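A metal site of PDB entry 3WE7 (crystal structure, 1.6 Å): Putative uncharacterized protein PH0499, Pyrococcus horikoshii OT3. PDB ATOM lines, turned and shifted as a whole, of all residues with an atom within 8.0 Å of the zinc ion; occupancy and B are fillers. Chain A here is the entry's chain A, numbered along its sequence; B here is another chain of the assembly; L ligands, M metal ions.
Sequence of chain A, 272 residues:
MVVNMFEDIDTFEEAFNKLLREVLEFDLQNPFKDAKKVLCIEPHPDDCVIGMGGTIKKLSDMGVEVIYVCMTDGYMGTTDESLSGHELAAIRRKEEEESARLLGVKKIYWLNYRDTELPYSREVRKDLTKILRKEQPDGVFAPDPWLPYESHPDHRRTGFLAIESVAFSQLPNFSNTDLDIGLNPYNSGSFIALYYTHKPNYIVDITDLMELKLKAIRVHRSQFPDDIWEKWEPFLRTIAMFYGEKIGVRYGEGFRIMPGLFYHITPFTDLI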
ATOM      1  N   GLU A  42     -20.858  13.099  16.485  1.00  0.00           N
ATOM      2  CA  GLU A  42     -20.418  12.119  17.502  1.00  0.00           C
ATOM      3  C   GLU A  42     -20.106  12.751  18.820  1.00  0.00           C
ATOM      4  O   GLU A  42     -19.457  13.789  18.832  1.00  0.00           O
ATOM      5  CB  GLU A  42     -19.105  11.348  17.077  1.00  0.00           C
ATOM      6  CG  GLU A  42     -17.964  12.201  16.471  1.00  0.00           C
ATOM      7  CD  GLU A  42     -16.764  11.358  15.958  1.00  0.00           C
ATOM      8  OE1 GLU A  42     -16.838  10.107  15.890  1.00  0.00           O
ATOM      9  OE2 GLU A  42     -15.705  12.030  15.777  1.00  0.00           O
ATOM     10  N   PRO A  43     -20.430  12.036  19.896  1.00  0.00           N
ATOM     11  CA  PRO A  43     -20.040  12.593  21.259  1.00  0.00           C
ATOM     12  C   PRO A  43     -18.509  12.642  21.433  1.00  0.00           C
ATOM     13  O   PRO A  43     -18.009  13.687  21.904  1.00  0.00           O
ATOM     14  CB  PRO A  43     -20.665  11.563  22.211  1.00  0.00           C
ATOM     15  CG  PRO A  43     -21.862  11.080  21.463  1.00  0.00           C
ATOM     16  CD  PRO A  43     -21.358  10.901  20.018  1.00  0.00           C
ATOM     17  N   HIS A  44     -17.812  11.562  20.979  1.00  0.00           N
ATOM     18  CA  HIS A  44     -16.402  11.359  21.245  1.00  0.00           C
ATOM     19  C   HIS A  44     -15.695  10.940  19.977  1.00  0.00           C
ATOM     20  O   HIS A  44     -16.368  10.401  19.098  1.00  0.00           O
ATOM     21  CB  HIS A  44     -16.170  10.245  22.246  1.00  0.00           C
ATOM     22  CG  HIS A  44     -16.985  10.406  23.556  1.00  0.00           C
ATOM     23  ND1 HIS A  44     -17.987   9.577  23.941  1.00  0.00           N
ATOM     24  CD2 HIS A  44     -16.873  11.425  24.542  1.00  0.00           C
ATOM     25  CE1 HIS A  44     -18.503  10.040  25.176  1.00  0.00           C
ATOM     26  NE2 HIS A  44     -17.796  11.155  25.519  1.00  0.00           N
ATOM     27  N   PRO A  45     -14.378  11.130  19.915  1.00  0.00           N
ATOM     28  CA  PRO A  45     -13.563  10.517  18.772  1.00  0.00           C
ATOM     29  C   PRO A  45     -13.800   9.015  18.799  1.00  0.00           C
ATOM     30  O   PRO A  45     -13.553   8.391  19.788  1.00  0.00           O
ATOM     31  CB  PRO A  45     -12.123  10.840  19.173  1.00  0.00           C
ATOM     32  CG  PRO A  45     -12.259  12.045  20.081  1.00  0.00           C
ATOM     33  CD  PRO A  45     -13.535  11.881  20.873  1.00  0.00           C
ATOM     34  N   ASP A  46     -14.333   8.502  17.700  1.00  0.00           N
ATOM     35  CA  ASP A  46     -14.573   7.041  17.501  1.00  0.00           C
ATOM     36  C   ASP A  46     -16.047   6.690  17.436  1.00  0.00           C
ATOM     37  O   ASP A  46     -16.404   5.577  17.015  1.00  0.00           O
ATOM     38  CB  ASP A  46     -13.846   6.058  18.454  1.00  0.00           C
ATOM     39  CG  ASP A  46     -14.414   5.988  19.827  1.00  0.00           C
ATOM     40  OD1 ASP A  46     -15.585   6.345  20.107  1.00  0.00           O
ATOM     41  OD2 ASP A  46     -13.692   5.399  20.669  1.00  0.00           O
ATOM     42  N   ASP A  47     -16.970   7.603  17.828  1.00  0.00           N
ATOM     43  CA  ASP A  47     -18.372   7.117  17.844  1.00  0.00           C
ATOM     44  C   ASP A  47     -19.018   7.021  16.445  1.00  0.00           C
ATOM     45  O   ASP A  47     -19.851   6.113  16.227  1.00  0.00           O
ATOM     46  CB  ASP A  47     -19.269   8.084  18.752  1.00  0.00           C
ATOM     47  CG  ASP A  47     -19.137   7.739  20.231  1.00  0.00           C
ATOM     48  OD1 ASP A  47     -19.380   6.574  20.626  1.00  0.00           O
ATOM     49  OD2 ASP A  47     -18.851   8.787  20.974  1.00  0.00           O
ATOM     50  N   CYS A  48     -18.591   7.861  15.553  1.00  0.00           N
ATOM     51  CA  CYS A  48     -19.130   7.815  14.164  1.00  0.00           C
ATOM     52  C   CYS A  48     -18.721   6.446  13.562  1.00  0.00           C
ATOM     53  O   CYS A  48     -19.595   5.755  12.971  1.00  0.00           O
ATOM     54  CB  CYS A  48     -18.608   8.913  13.230  1.00  0.00           C
ATOM     55  SG  CYS A  48     -19.428  10.482  13.589  1.00  0.00           S
ATOM     56  N   ILE A  50     -17.668   3.583  15.209  1.00  0.00           N
ATOM     57  CA  ILE A  50     -18.350   2.524  15.875  1.00  0.00           C
ATOM     58  C   ILE A  50     -19.819   2.360  15.559  1.00  0.00           C
ATOM     59  O   ILE A  50     -20.309   1.239  15.316  1.00  0.00           O
ATOM     60  CB  ILE A  50     -18.127   2.663  17.440  1.00  0.00           C
ATOM     61  CG1 ILE A  50     -16.678   2.515  17.759  1.00  0.00           C
ATOM     62  CG2 ILE A  50     -18.910   1.624  18.219  1.00  0.00           C
ATOM     63  CD1 ILE A  50     -16.419   2.951  19.241  1.00  0.00           C
ATOM     64  N   THR A  72     -16.759  16.394  21.755  1.00  0.00           N
ATOM     65  CA  THR A  72     -15.822  16.489  22.848  1.00  0.00           C
ATOM     66  C   THR A  72     -14.433  16.030  22.427  1.00  0.00           C
ATOM     67  O   THR A  72     -14.244  15.481  21.348  1.00  0.00           O
ATOM     68  CB  THR A  72     -16.171  15.618  24.062  1.00  0.00           C
ATOM     69  OG1 THR A  72     -16.008  14.184  23.831  1.00  0.00           O
ATOM     70  CG2 THR A  72     -17.624  15.865  24.548  1.00  0.00           C
ATOM     71  N   ARG A  92      -5.876  11.442  20.243  1.00  0.00           N
ATOM     72  CA  ARG A  92      -7.128  10.999  19.664  1.00  0.00           C
ATOM     73  C   ARG A  92      -7.552  11.788  18.455  1.00  0.00           C
ATOM     74  O   ARG A  92      -8.288  11.286  17.576  1.00  0.00           O
ATOM     75  CB  ARG A  92      -8.278  10.931  20.713  1.00  0.00           C
ATOM     76  CG  ARG A  92      -7.968   9.982  21.803  1.00  0.00           C
ATOM     77  CD  ARG A  92      -9.116   9.842  22.778  1.00  0.00           C
ATOM     78  NE  ARG A  92     -10.272   9.143  22.211  1.00  0.00           N
ATOM     79  CZ  ARG A  92     -11.346   8.826  22.989  1.00  0.00           C
ATOM     80  NH1 ARG A  92     -11.371   9.174  24.343  1.00  0.00           N
ATOM     81  NH2 ARG A  92     -12.373   8.172  22.462  1.00  0.00           N
ATOM     82  N   ASP A 115     -14.443  15.888  27.394  1.00  0.00           N
ATOM     83  CA  ASP A 115     -15.101  14.612  27.558  1.00  0.00           C
ATOM     84  C   ASP A 115     -15.581  14.454  29.047  1.00  0.00           C
ATOM     85  O   ASP A 115     -14.829  14.811  30.041  1.00  0.00           O
ATOM     86  CB  ASP A 115     -13.949  13.568  27.300  1.00  0.00           C
ATOM     87  CG  ASP A 115     -14.327  12.174  27.453  1.00  0.00           C
ATOM     88  OD1 ASP A 115     -15.466  11.758  27.621  1.00  0.00           O
ATOM     89  OD2 ASP A 115     -13.335  11.344  27.321  1.00  0.00           O
ATOM     90  N   PRO A 143     -26.574  10.245  17.808  1.00  0.00           N
ATOM     91  CA  PRO A 143     -27.007   9.158  18.656  1.00  0.00           C
ATOM     92  C   PRO A 143     -28.463   9.372  19.095  1.00  0.00           C
ATOM     93  O   PRO A 143     -28.888  10.533  19.266  1.00  0.00           O
ATOM     94  CB  PRO A 143     -26.138   9.339  19.944  1.00  0.00           C
ATOM     95  CG  PRO A 143     -24.875  10.094  19.423  1.00  0.00           C
ATOM     96  CD  PRO A 143     -25.424  11.034  18.355  1.00  0.00           C
ATOM     97  N   GLU A 150     -28.584   3.991  28.407  1.00  0.00           N
ATOM     98  CA  GLU A 150     -27.427   4.788  28.008  1.00  0.00           C
ATOM     99  C   GLU A 150     -26.950   5.695  29.129  1.00  0.00           C
ATOM    100  O   GLU A 150     -27.682   6.651  29.477  1.00  0.00           O
ATOM    101  CB  GLU A 150     -27.658   5.563  26.690  1.00  0.00           C
ATOM    102  CG  GLU A 150     -26.478   6.544  26.421  1.00  0.00           C
ATOM    103  CD  GLU A 150     -25.176   5.777  26.248  1.00  0.00           C
ATOM    104  OE1 GLU A 150     -25.093   4.949  25.273  1.00  0.00           O
ATOM    105  OE2 GLU A 150     -24.299   5.953  27.084  1.00  0.00           O
ATOM    106  N   HIS A 152     -23.986   7.391  29.516  1.00  0.00           N
ATOM    107  CA  HIS A 152     -22.966   8.429  29.299  1.00  0.00           C
ATOM    108  C   HIS A 152     -23.644   9.720  28.986  1.00  0.00           C
ATOM    109  O   HIS A 152     -24.318   9.844  27.978  1.00  0.00           O
ATOM    110  CB  HIS A 152     -22.020   8.055  28.146  1.00  0.00           C
ATOM    111  CG  HIS A 152     -20.722   8.724  28.236  1.00  0.00           C
ATOM    112  ND1 HIS A 152     -20.626  10.087  28.432  1.00  0.00           N
ATOM    113  CD2 HIS A 152     -19.407   8.217  28.237  1.00  0.00           C
ATOM    114  CE1 HIS A 152     -19.350  10.426  28.497  1.00  0.00           C
ATOM    115  NE2 HIS A 152     -18.588   9.277  28.409  1.00  0.00           N
ATOM    116  N   ASP A 154     -22.538  12.425  27.857  1.00  0.00           N
ATOM    117  CA  ASP A 154     -22.186  13.061  26.637  1.00  0.00           C
ATOM    118  C   ASP A 154     -22.986  12.452  25.470  1.00  0.00           C
ATOM    119  O   ASP A 154     -23.243  13.180  24.521  1.00  0.00           O
ATOM    120  CB  ASP A 154     -20.703  12.827  26.339  1.00  0.00           C
ATOM    121  CG  ASP A 154     -19.715  13.588  27.210  1.00  0.00           C
ATOM    122  OD1 ASP A 154     -18.526  13.127  27.231  1.00  0.00           O
ATOM    123  OD2 ASP A 154     -20.052  14.521  28.004  1.00  0.00           O
ATOM    124  N   HIS A 155     -23.385  11.216  25.577  1.00  0.00           N
ATOM    125  CA  HIS A 155     -24.147  10.551  24.495  1.00  0.00           C
ATOM    126  C   HIS A 155     -25.559  11.063  24.529  1.00  0.00           C
ATOM    127  O   HIS A 155     -26.088  11.506  23.471  1.00  0.00           O
ATOM    128  CB  HIS A 155     -24.084   9.037  24.579  1.00  0.00           C
ATOM    129  CG  HIS A 155     -22.852   8.487  24.014  1.00  0.00           C
ATOM    130  ND1 HIS A 155     -22.886   7.374  23.225  1.00  0.00           N
ATOM    131  CD2 HIS A 155     -21.553   8.904  24.080  1.00  0.00           C
ATOM    132  CE1 HIS A 155     -21.629   7.106  22.791  1.00  0.00           C
ATOM    133  NE2 HIS A 155     -20.811   8.017  23.301  1.00  0.00           N
ATOM    134  N   THR A 158     -25.562  14.781  23.367  1.00  0.00           N
ATOM    135  CA  THR A 158     -25.330  15.039  21.991  1.00  0.00           C
ATOM    136  C   THR A 158     -26.591  14.727  21.167  1.00  0.00           C
ATOM    137  O   THR A 158     -26.904  15.459  20.240  1.00  0.00           O
ATOM    138  CB  THR A 158     -24.237  14.077  21.485  1.00  0.00           C
ATOM    139  OG1 THR A 158     -22.966  14.400  22.076  1.00  0.00           O
ATOM    140  CG2 THR A 158     -24.081  14.284  20.017  1.00  0.00           C
ATOM    141  N   TYR A 195     -28.432   6.896  15.144  1.00  0.00           N
ATOM    142  CA  TYR A 195     -27.792   5.673  15.351  1.00  0.00           C
ATOM    143  C   TYR A 195     -27.661   5.366  16.786  1.00  0.00           C
ATOM    144  O   TYR A 195     -28.197   6.135  17.617  1.00  0.00           O
ATOM    145  CB  TYR A 195     -26.417   5.657  14.613  1.00  0.00           C
ATOM    146  CG  TYR A 195     -25.380   6.735  15.056  1.00  0.00           C
ATOM    147  CD1 TYR A 195     -25.373   8.054  14.546  1.00  0.00           C
ATOM    148  CD2 TYR A 195     -24.484   6.380  16.047  1.00  0.00           C
ATOM    149  CE1 TYR A 195     -24.376   9.035  14.930  1.00  0.00           C
ATOM    150  CE2 TYR A 195     -23.508   7.341  16.444  1.00  0.00           C
ATOM    151  CZ  TYR A 195     -23.461   8.600  15.918  1.00  0.00           C
ATOM    152  OH  TYR A 195     -22.468   9.457  16.406  1.00  0.00           O
ATOM    153  N   TYR A 196     -27.000   4.267  17.101  1.00  0.00           N
ATOM    154  CA  TYR A 196     -26.979   3.769  18.520  1.00  0.00           C
ATOM    155  C   TYR A 196     -28.380   3.691  19.038  1.00  0.00           C
ATOM    156  O   TYR A 196     -28.694   4.259  20.151  1.00  0.00           O
ATOM    157  CB  TYR A 196     -26.143   4.720  19.418  1.00  0.00           C
ATOM    158  CG  TYR A 196     -24.635   4.644  19.284  1.00  0.00           C
ATOM    159  CD1 TYR A 196     -23.988   3.476  18.872  1.00  0.00           C
ATOM    160  CD2 TYR A 196     -23.865   5.736  19.617  1.00  0.00           C
ATOM    161  CE1 TYR A 196     -22.577   3.408  18.792  1.00  0.00           C
ATOM    162  CE2 TYR A 196     -22.467   5.711  19.544  1.00  0.00           C
ATOM    163  CZ  TYR A 196     -21.810   4.541  19.181  1.00  0.00           C
ATOM    164  OH  TYR A 196     -20.483   4.580  19.235  1.00  0.00           O
ATOM    165  N   GLN A 223      -7.907   3.658  22.599  1.00  0.00           N
ATOM    166  CA  GLN A 223      -9.179   3.149  23.155  1.00  0.00           C
ATOM    167  C   GLN A 223      -9.262   1.627  23.136  1.00  0.00           C
ATOM    168  O   GLN A 223     -10.023   1.054  23.896  1.00  0.00           O
ATOM    169  CB  GLN A 223     -10.326   3.701  22.306  1.00  0.00           C
ATOM    170  CG  GLN A 223     -10.332   5.187  22.243  1.00  0.00           C
ATOM    171  CD  GLN A 223     -10.376   5.760  23.705  1.00  0.00           C
ATOM    172  OE1 GLN A 223     -11.409   5.562  24.409  1.00  0.00           O
ATOM    173  NE2 GLN A 223      -9.246   6.372  24.182  1.00  0.00           N
ATOM    174  N   TRP A 232     -14.419  -6.059  23.344  1.00  0.00           N
ATOM    175  CA  TRP A 232     -15.128  -5.184  22.371  1.00  0.00           C
ATOM    176  C   TRP A 232     -15.398  -5.778  21.016  1.00  0.00           C
ATOM    177  O   TRP A 232     -16.414  -5.477  20.369  1.00  0.00           O
ATOM    178  CB  TRP A 232     -14.396  -3.836  22.226  1.00  0.00           C
ATOM    179  CG  TRP A 232     -14.911  -2.905  23.322  1.00  0.00           C
ATOM    180  CD1 TRP A 232     -14.622  -2.909  24.677  1.00  0.00           C
ATOM    181  CD2 TRP A 232     -15.877  -1.830  23.155  1.00  0.00           C
ATOM    182  NE1 TRP A 232     -15.290  -1.914  25.340  1.00  0.00           N
ATOM    183  CE2 TRP A 232     -16.089  -1.246  24.493  1.00  0.00           C
ATOM    184  CE3 TRP A 232     -16.597  -1.336  22.081  1.00  0.00           C
ATOM    185  CZ2 TRP A 232     -16.988  -0.209  24.720  1.00  0.00           C
ATOM    186  CZ3 TRP A 232     -17.488  -0.262  22.314  1.00  0.00           C
ATOM    187  CH2 TRP A 232     -17.631   0.302  23.611  1.00  0.00           C
ATOM    188  N   HIS B 264     -23.887   1.262  27.964  1.00  0.00           N
ATOM    189  CA  HIS B 264     -23.459   2.151  26.926  1.00  0.00           C
ATOM    190  C   HIS B 264     -23.638   1.519  25.561  1.00  0.00           C
ATOM    191  O   HIS B 264     -23.210   0.356  25.299  1.00  0.00           O
ATOM    192  CB  HIS B 264     -22.010   2.490  27.214  1.00  0.00           C
ATOM    193  CG  HIS B 264     -21.434   3.617  26.365  1.00  0.00           C
ATOM    194  ND1 HIS B 264     -22.005   4.843  26.265  1.00  0.00           N
ATOM    195  CD2 HIS B 264     -20.212   3.691  25.655  1.00  0.00           C
ATOM    196  CE1 HIS B 264     -21.226   5.644  25.510  1.00  0.00           C
ATOM    197  NE2 HIS B 264     -20.100   4.918  25.170  1.00  0.00           N
ATOM    198  N   ILE B 265     -24.223   2.324  24.689  1.00  0.00           N
ATOM    199  CA  ILE B 265     -24.443   2.039  23.230  1.00  0.00           C
ATOM    200  C   ILE B 265     -25.117   0.710  22.947  1.00  0.00           C
ATOM    201  O   ILE B 265     -25.028   0.187  21.830  1.00  0.00           O
ATOM    202  CB  ILE B 265     -23.165   2.212  22.316  1.00  0.00           C
ATOM    203  CG1 ILE B 265     -22.095   1.148  22.597  1.00  0.00           C
ATOM    204  CG2 ILE B 265     -22.620   3.680  22.550  1.00  0.00           C
ATOM    205  CD1 ILE B 265     -21.081   1.103  21.406  1.00  0.00           C
HETATM  206  C1  LIG L   1     -17.408   5.921  22.975  1.00  0.00           C
HETATM  207  O1  LIG L   1     -16.572   6.764  22.506  1.00  0.00           O
HETATM  208  O2  LIG L   1     -18.329   6.310  23.733  1.00  0.00           O
HETATM  209  C2  LIG L   1     -17.312   4.418  22.694  1.00  0.00           C
HETATM  210 ZN    ZN M   1     -18.763   7.950  22.909  1.00  0.00          ZN
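OD1 of Asp 115 sits at hydrogen-bond distance from NE2 of His 44 (3.2 Å).
The side-chain carboxylate of Glu 42 is in hydrogen-bond range of the backbone NH of Asp 47, at 3.2 Å.
The side-chain carboxylate (OD1) of Asp 154 lies within hydrogen-bond range of a ring nitrogen (NE2) of His 44 (2.7 Å).
OH of Tyr 196 lies within hydrogen-bond range of OD1 of Asp 47 (2.7 Å).
The zinc ion is bound by an oxygen (O2) of the ligand (1.9 Å), a ring nitrogen (ND1) of His 44 (2.1 Å), a ring nitrogen (NE2) of His 155 (2.1 Å), the side-chain carboxylate (OD2) of Asp 47 (2.1 Å) and an oxygen (O1) of the ligand (2.5 Å).
Slightly farther from the zinc ion lies the side-chain carboxylate (OD1) of Asp 47 (2.7 Å).
Three residues have an atom within 4 Å of the zinc ion: His 44, Asp 47 and His 155.
Along chain A the residues within 4 Å of the zinc ion span positions 44 to 155.
The nearest printed residue that does not touch the zinc ion is His 264 of chain B (4.01 Å).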
